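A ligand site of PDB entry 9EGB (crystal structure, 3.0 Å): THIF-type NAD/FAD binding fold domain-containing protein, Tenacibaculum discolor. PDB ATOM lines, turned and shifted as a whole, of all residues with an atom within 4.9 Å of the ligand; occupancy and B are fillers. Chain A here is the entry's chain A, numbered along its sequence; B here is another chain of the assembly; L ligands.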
ATOM      1  N   GLY A  46      -3.881   6.108  35.657  1.00  0.00           N
ATOM      2  CA  GLY A  46      -3.381   7.171  34.827  1.00  0.00           C
ATOM      3  C   GLY A  46      -4.164   7.233  33.538  1.00  0.00           C
ATOM      4  O   GLY A  46      -5.256   7.808  33.486  1.00  0.00           O
ATOM      5  N   ILE A  47      -3.645   6.601  32.484  1.00  0.00           N
ATOM      6  CA  ILE A  47      -4.450   6.381  31.291  1.00  0.00           C
ATOM      7  C   ILE A  47      -5.752   5.670  31.654  1.00  0.00           C
ATOM      8  O   ILE A  47      -6.792   5.854  31.001  1.00  0.00           O
ATOM      9  CB  ILE A  47      -3.628   5.599  30.250  1.00  0.00           C
ATOM     10  CG1 ILE A  47      -4.424   5.337  28.988  1.00  0.00           C
ATOM     11  CG2 ILE A  47      -3.250   4.254  30.797  1.00  0.00           C
ATOM     12  CD1 ILE A  47      -3.612   4.567  27.996  1.00  0.00           C
ATOM     13  N   ASN A 131      -4.453  -3.988  32.315  1.00  0.00           N
ATOM     14  CA  ASN A 131      -3.090  -3.811  32.810  1.00  0.00           C
ATOM     15  C   ASN A 131      -2.602  -2.478  32.265  1.00  0.00           C
ATOM     16  O   ASN A 131      -2.165  -2.375  31.116  1.00  0.00           O
ATOM     17  CB  ASN A 131      -2.206  -4.964  32.370  1.00  0.00           C
ATOM     18  CG  ASN A 131      -0.825  -4.919  32.997  1.00  0.00           C
ATOM     19  OD1 ASN A 131      -0.325  -3.861  33.380  1.00  0.00           O
ATOM     20  ND2 ASN A 131      -0.200  -6.075  33.107  1.00  0.00           N
ATOM     21  N   ALA A 132      -2.657  -1.446  33.099  1.00  0.00           N
ATOM     22  CA  ALA A 132      -2.110  -0.140  32.779  1.00  0.00           C
ATOM     23  C   ALA A 132      -1.004   0.207  33.753  1.00  0.00           C
ATOM     24  O   ALA A 132      -0.889   1.343  34.210  1.00  0.00           O
ATOM     25  CB  ALA A 132      -3.199   0.936  32.793  1.00  0.00           C
ATOM     26  N   LEU A 133      -0.173  -0.790  34.081  1.00  0.00           N
ATOM     27  CA  LEU A 133       0.849  -0.622  35.103  1.00  0.00           C
ATOM     28  C   LEU A 133       2.170  -0.155  34.522  1.00  0.00           C
ATOM     29  O   LEU A 133       2.584  -0.613  33.445  1.00  0.00           O
ATOM     30  CB  LEU A 133       1.065  -1.934  35.875  1.00  0.00           C
ATOM     31  CG  LEU A 133      -0.167  -2.480  36.609  1.00  0.00           C
ATOM     32  CD1 LEU A 133       0.063  -3.900  37.133  1.00  0.00           C
ATOM     33  CD2 LEU A 133      -0.594  -1.537  37.723  1.00  0.00           C
ATOM     34  N   ASP A 134       2.777   0.827  35.184  1.00  0.00           N
ATOM     35  CA  ASP A 134       4.138   1.235  34.874  1.00  0.00           C
ATOM     36  C   ASP A 134       5.080   0.043  34.956  1.00  0.00           C
ATOM     37  O   ASP A 134       5.029  -0.763  35.890  1.00  0.00           O
ATOM     38  CB  ASP A 134       4.609   2.306  35.863  1.00  0.00           C
ATOM     39  CG  ASP A 134       3.812   3.599  35.758  1.00  0.00           C
ATOM     40  OD1 ASP A 134       2.997   3.728  34.824  1.00  0.00           O
ATOM     41  OD2 ASP A 134       3.985   4.475  36.640  1.00  0.00           O
ATOM     42  N   PHE A 135       5.978  -0.046  33.981  1.00  0.00           N
ATOM     43  CA  PHE A 135       6.981  -1.106  33.911  1.00  0.00           C
ATOM     44  C   PHE A 135       8.160  -0.854  34.852  1.00  0.00           C
ATOM     45  O   PHE A 135       9.072  -1.684  34.937  1.00  0.00           O
ATOM     46  CB  PHE A 135       7.455  -1.263  32.466  1.00  0.00           C
ATOM     47  CG  PHE A 135       6.491  -2.038  31.609  1.00  0.00           C
ATOM     48  CD1 PHE A 135       6.450  -3.432  31.680  1.00  0.00           C
ATOM     49  CD2 PHE A 135       5.614  -1.388  30.764  1.00  0.00           C
ATOM     50  CE1 PHE A 135       5.566  -4.165  30.906  1.00  0.00           C
ATOM     51  CE2 PHE A 135       4.712  -2.116  29.985  1.00  0.00           C
ATOM     52  CZ  PHE A 135       4.695  -3.497  30.054  1.00  0.00           C
ATOM     53  N   HIS A 156      -4.151  -4.482  27.470  1.00  0.00           N
ATOM     54  CA  HIS A 156      -2.972  -3.633  27.613  1.00  0.00           C
ATOM     55  C   HIS A 156      -3.181  -2.407  26.749  1.00  0.00           C
ATOM     56  O   HIS A 156      -3.068  -2.491  25.519  1.00  0.00           O
ATOM     57  CB  HIS A 156      -1.648  -4.316  27.208  1.00  0.00           C
ATOM     58  CG  HIS A 156      -1.049  -5.192  28.268  1.00  0.00           C
ATOM     59  ND1 HIS A 156      -0.034  -4.735  29.083  1.00  0.00           N
ATOM     60  CD2 HIS A 156      -1.303  -6.460  28.666  1.00  0.00           C
ATOM     61  CE1 HIS A 156       0.323  -5.690  29.924  1.00  0.00           C
ATOM     62  NE2 HIS A 156      -0.443  -6.741  29.703  1.00  0.00           N
ATOM     63  N   PRO A 157      -3.572  -1.288  27.336  1.00  0.00           N
ATOM     64  CA  PRO A 157      -3.686  -0.041  26.569  1.00  0.00           C
ATOM     65  C   PRO A 157      -2.398   0.768  26.593  1.00  0.00           C
ATOM     66  O   PRO A 157      -1.695   0.852  27.597  1.00  0.00           O
ATOM     67  CB  PRO A 157      -4.833   0.689  27.285  1.00  0.00           C
ATOM     68  CG  PRO A 157      -4.720   0.261  28.685  1.00  0.00           C
ATOM     69  CD  PRO A 157      -4.253  -1.191  28.638  1.00  0.00           C
ATOM     70  N   TYR A 158      -2.070   1.362  25.451  1.00  0.00           N
ATOM     71  CA  TYR A 158      -0.896   2.206  25.305  1.00  0.00           C
ATOM     72  C   TYR A 158      -1.300   3.506  24.628  1.00  0.00           C
ATOM     73  O   TYR A 158      -2.125   3.511  23.717  1.00  0.00           O
ATOM     74  CB  TYR A 158       0.197   1.525  24.476  1.00  0.00           C
ATOM     75  CG  TYR A 158       0.686   0.284  25.118  1.00  0.00           C
ATOM     76  CD1 TYR A 158       0.068  -0.943  24.917  1.00  0.00           C
ATOM     77  CD2 TYR A 158       1.845   0.316  25.891  1.00  0.00           C
ATOM     78  CE1 TYR A 158       0.547  -2.083  25.520  1.00  0.00           C
ATOM     79  CE2 TYR A 158       2.338  -0.822  26.485  1.00  0.00           C
ATOM     80  CZ  TYR A 158       1.692  -2.013  26.295  1.00  0.00           C
ATOM     81  OH  TYR A 158       2.179  -3.134  26.924  1.00  0.00           O
ATOM     82  N   ASN A 159      -0.636   4.581  25.044  1.00  0.00           N
ATOM     83  CA  ASN A 159      -0.866   5.930  24.542  1.00  0.00           C
ATOM     84  C   ASN A 159       0.264   6.213  23.556  1.00  0.00           C
ATOM     85  O   ASN A 159       1.388   6.525  23.943  1.00  0.00           O
ATOM     86  CB  ASN A 159      -0.898   6.940  25.695  1.00  0.00           C
ATOM     87  CG  ASN A 159      -1.247   8.354  25.254  1.00  0.00           C
ATOM     88  OD1 ASN A 159      -0.740   8.864  24.239  1.00  0.00           O
ATOM     89  ND2 ASN A 159      -2.107   9.016  26.031  1.00  0.00           N
ATOM     90  N   LEU A 160      -0.035   6.116  22.271  1.00  0.00           N
ATOM     91  CA  LEU A 160       0.992   6.410  21.283  1.00  0.00           C
ATOM     92  C   LEU A 160       0.874   7.834  20.777  1.00  0.00           C
ATOM     93  O   LEU A 160       1.184   8.123  19.620  1.00  0.00           O
ATOM     94  CB  LEU A 160       0.922   5.407  20.121  1.00  0.00           C
ATOM     95  CG  LEU A 160       0.965   3.911  20.422  1.00  0.00           C
ATOM     96  CD1 LEU A 160       1.533   3.143  19.240  1.00  0.00           C
ATOM     97  CD2 LEU A 160       1.757   3.608  21.682  1.00  0.00           C
ATOM     98  N   GLU A 188       7.415  -0.533  27.955  1.00  0.00           N
ATOM     99  CA  GLU A 188       6.507  -0.184  26.878  1.00  0.00           C
ATOM    100  C   GLU A 188       7.221   0.098  25.560  1.00  0.00           C
ATOM    101  O   GLU A 188       6.602  -0.059  24.504  1.00  0.00           O
ATOM    102  CB  GLU A 188       5.670   1.028  27.309  1.00  0.00           C
ATOM    103  CG  GLU A 188       6.474   2.270  27.693  1.00  0.00           C
ATOM    104  CD  GLU A 188       6.967   2.262  29.152  1.00  0.00           C
ATOM    105  OE1 GLU A 188       6.897   1.201  29.810  1.00  0.00           O
ATOM    106  OE2 GLU A 188       7.418   3.323  29.637  1.00  0.00           O
ATOM    107  N   LEU A 189       8.490   0.489  25.600  1.00  0.00           N
ATOM    108  CA  LEU A 189       9.208   0.729  24.347  1.00  0.00           C
ATOM    109  C   LEU A 189       9.345  -0.553  23.522  1.00  0.00           C
ATOM    110  O   LEU A 189       9.384  -0.490  22.289  1.00  0.00           O
ATOM    111  CB  LEU A 189      10.573   1.353  24.641  1.00  0.00           C
ATOM    112  CG  LEU A 189      11.202   2.116  23.461  1.00  0.00           C
ATOM    113  CD1 LEU A 189      10.258   3.242  23.029  1.00  0.00           C
ATOM    114  CD2 LEU A 189      12.571   2.681  23.807  1.00  0.00           C
ATOM    115  N   VAL A 192       5.901  -1.067  21.686  1.00  0.00           N
ATOM    116  CA  VAL A 192       5.704  -0.116  20.606  1.00  0.00           C
ATOM    117  C   VAL A 192       6.680  -0.413  19.463  1.00  0.00           C
ATOM    118  O   VAL A 192       6.308  -0.316  18.286  1.00  0.00           O
ATOM    119  CB  VAL A 192       5.867   1.304  21.184  1.00  0.00           C
ATOM    120  CG1 VAL A 192       5.944   2.349  20.108  1.00  0.00           C
ATOM    121  CG2 VAL A 192       4.715   1.596  22.118  1.00  0.00           C
ATOM    122  N   ILE A 212       8.355   9.041  16.334  1.00  0.00           N
ATOM    123  CA  ILE A 212       8.359   9.297  17.771  1.00  0.00           C
ATOM    124  C   ILE A 212       9.192   8.274  18.527  1.00  0.00           C
ATOM    125  O   ILE A 212       9.822   8.623  19.538  1.00  0.00           O
ATOM    126  CB  ILE A 212       6.922   9.371  18.310  1.00  0.00           C
ATOM    127  CG1 ILE A 212       6.937   9.955  19.728  1.00  0.00           C
ATOM    128  CG2 ILE A 212       6.242   8.017  18.271  1.00  0.00           C
ATOM    129  CD1 ILE A 212       7.427  11.378  19.780  1.00  0.00           C
ATOM    130  N   ILE A 213       9.231   7.021  18.075  1.00  0.00           N
ATOM    131  CA  ILE A 213      10.138   6.062  18.690  1.00  0.00           C
ATOM    132  C   ILE A 213      11.568   6.560  18.540  1.00  0.00           C
ATOM    133  O   ILE A 213      12.334   6.598  19.510  1.00  0.00           O
ATOM    134  CB  ILE A 213       9.945   4.675  18.058  1.00  0.00           C
ATOM    135  CG1 ILE A 213       8.577   4.112  18.429  1.00  0.00           C
ATOM    136  CG2 ILE A 213      11.013   3.712  18.547  1.00  0.00           C
ATOM    137  CD1 ILE A 213       8.278   2.815  17.713  1.00  0.00           C
ATOM    138  N   PHE A 216      12.369   9.649  20.726  1.00  0.00           N
ATOM    139  CA  PHE A 216      12.422   9.317  22.148  1.00  0.00           C
ATOM    140  C   PHE A 216      13.730   8.619  22.510  1.00  0.00           C
ATOM    141  O   PHE A 216      14.331   8.921  23.549  1.00  0.00           O
ATOM    142  CB  PHE A 216      11.193   8.477  22.530  1.00  0.00           C
ATOM    143  CG  PHE A 216      11.220   7.972  23.951  1.00  0.00           C
ATOM    144  CD1 PHE A 216      11.323   8.857  25.018  1.00  0.00           C
ATOM    145  CD2 PHE A 216      11.094   6.619  24.245  1.00  0.00           C
ATOM    146  CE1 PHE A 216      11.340   8.412  26.330  1.00  0.00           C
ATOM    147  CE2 PHE A 216      11.100   6.163  25.549  1.00  0.00           C
ATOM    148  CZ  PHE A 216      11.224   7.064  26.590  1.00  0.00           C
ATOM    149  N   PRO A 225       8.144   8.348  28.662  1.00  0.00           N
ATOM    150  CA  PRO A 225       7.617   8.567  27.299  1.00  0.00           C
ATOM    151  C   PRO A 225       6.582   9.669  27.254  1.00  0.00           C
ATOM    152  O   PRO A 225       5.756   9.821  28.167  1.00  0.00           O
ATOM    153  CB  PRO A 225       6.967   7.214  26.962  1.00  0.00           C
ATOM    154  CG  PRO A 225       7.564   6.236  27.912  1.00  0.00           C
ATOM    155  CD  PRO A 225       7.876   6.990  29.157  1.00  0.00           C
ATOM    156  N   PRO A 226       6.595  10.478  26.189  1.00  0.00           N
ATOM    157  CA  PRO A 226       5.534  11.472  26.001  1.00  0.00           C
ATOM    158  C   PRO A 226       4.204  10.808  25.665  1.00  0.00           C
ATOM    159  O   PRO A 226       4.148   9.731  25.044  1.00  0.00           O
ATOM    160  CB  PRO A 226       6.060  12.322  24.839  1.00  0.00           C
ATOM    161  CG  PRO A 226       6.958  11.436  24.096  1.00  0.00           C
ATOM    162  CD  PRO A 226       7.604  10.543  25.128  1.00  0.00           C
ATOM    163  N   GLN A 227       3.119  11.478  26.039  1.00  0.00           N
ATOM    164  CA  GLN A 227       1.773  11.025  25.735  1.00  0.00           C
ATOM    165  C   GLN A 227       0.890  12.248  25.503  1.00  0.00           C
ATOM    166  O   GLN A 227       1.201  13.341  25.982  1.00  0.00           O
ATOM    167  CB  GLN A 227       1.206  10.174  26.889  1.00  0.00           C
ATOM    168  CG  GLN A 227       2.152   9.132  27.417  1.00  0.00           C
ATOM    169  CD  GLN A 227       1.524   8.277  28.484  1.00  0.00           C
ATOM    170  OE1 GLN A 227       0.343   8.409  28.794  1.00  0.00           O
ATOM    171  NE2 GLN A 227       2.326   7.420  29.099  1.00  0.00           N
ATOM    172  N   TYR B  26       6.271  15.208  20.540  1.00  0.00           N
ATOM    173  CA  TYR B  26       5.086  15.329  19.677  1.00  0.00           C
ATOM    174  C   TYR B  26       4.847  16.769  19.277  1.00  0.00           C
ATOM    175  O   TYR B  26       4.522  17.062  18.117  1.00  0.00           O
ATOM    176  CB  TYR B  26       3.858  14.788  20.399  1.00  0.00           C
ATOM    177  CG  TYR B  26       3.847  13.290  20.625  1.00  0.00           C
ATOM    178  CD1 TYR B  26       3.741  12.396  19.562  1.00  0.00           C
ATOM    179  CD2 TYR B  26       3.879  12.767  21.899  1.00  0.00           C
ATOM    180  CE1 TYR B  26       3.707  11.026  19.779  1.00  0.00           C
ATOM    181  CE2 TYR B  26       3.847  11.411  22.121  1.00  0.00           C
ATOM    182  CZ  TYR B  26       3.757  10.546  21.058  1.00  0.00           C
ATOM    183  OH  TYR B  26       3.709   9.191  21.299  1.00  0.00           O
HETATM  184  C1  LIG L   1       1.102   2.499  30.912  1.00  0.00           C
HETATM  185  C2  LIG L   1       1.248   0.114  29.972  1.00  0.00           C
HETATM  186  C3  LIG L   1       7.930   6.726  22.410  1.00  0.00           C
HETATM  187  C4  LIG L   1       6.464   6.385  22.199  1.00  0.00           C
HETATM  188  C5  LIG L   1       5.987   5.175  23.024  1.00  0.00           C
HETATM  189  C6  LIG L   1       5.031   5.580  24.142  1.00  0.00           C
HETATM  190  C7  LIG L   1       4.982   4.565  25.253  1.00  0.00           C
HETATM  191  C8  LIG L   1       3.584   4.222  25.828  1.00  0.00           C
HETATM  192  C9  LIG L   1       3.346   4.792  27.231  1.00  0.00           C
HETATM  193  C10 LIG L   1       2.012   4.428  27.940  1.00  0.00           C
HETATM  194  C11 LIG L   1       0.846   3.863  30.208  1.00  0.00           C
HETATM  195  C12 LIG L   1       0.590   4.999  31.350  1.00  0.00           C
HETATM  196  C13 LIG L   1       0.350   1.333  30.209  1.00  0.00           C
HETATM  197  C14 LIG L   1       0.442  -1.224  29.902  1.00  0.00           C
HETATM  198  N1  LIG L   1       2.044   4.233  29.349  1.00  0.00           N
HETATM  199  N2  LIG L   1       1.389  -2.388  29.837  1.00  0.00           N
HETATM  200  O1  LIG L   1       1.008   4.292  27.254  1.00  0.00           O
HETATM  201  O2  LIG L   1       1.532   5.803  31.551  1.00  0.00           O
HETATM  202  O3  LIG L   1      -0.511   5.027  31.937  1.00  0.00           O
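The backbone NH (N) of Asn 159 is in hydrogen-bond range of an oxygen (O1) of the ligand, at 2.8 Å. A nitrogen (N2) of the ligand sits at hydrogen-bond distance from a ring nitrogen (ND1) of His 156, 2.8 Å away. An oxygen (O2) of the ligand lies within hydrogen-bond range of the side-chain amide nitrogen of Gln 227 (3.0 Å). A nitrogen (N2) of the ligand lies within hydrogen-bond range of the side-chain hydroxyl (OH) of Tyr 158 (3.1 Å).
CG2 of Ile 47 touches O3 of the ligand, at 3.1 Å. Asn 131 touches the ligand. CA of Ala 132 touches C13 of the ligand, 3.9 Å away. Leu 133 touches the ligand. Phe 135 touches the ligand (CE2 to N2, 3.3 Å). Pro 157 touches the ligand. Glu 188 touches the ligand. Val 192 touches the ligand (CG2 to C5, 3.9 Å). O of Ile 212 touches C3 of the ligand, 3.9 Å away. Phe 216 touches the ligand. CB of Pro 225 touches C7 of the ligand, at 3.7 Å. Hydrophobic or aromatic side chains within 4 Å of the ligand: Ile 47, Phe 135, His 156, Tyr 158, Val 192, Phe 216 and Pro 225. Of the 22 residues printed, 15 come within 4 Å of the ligand. The nearest printed residue that does not touch the ligand is Tyr 26 of chain B (4.03 Å).
A ring nitrogen (NE2) of His 156 lies close to the side-chain amide nitrogen (ND2) of Asn 131 (3.5 Å). A ring nitrogen (ND1) of His 156 sits at hydrogen-bond distance from the side-chain hydroxyl (OH) of Tyr 158 (3.5 Å). The backbone NH (N) of Leu 133 is in hydrogen-bond range of the side-chain amide oxygen (OD1) of Asn 131 (3.2 Å).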
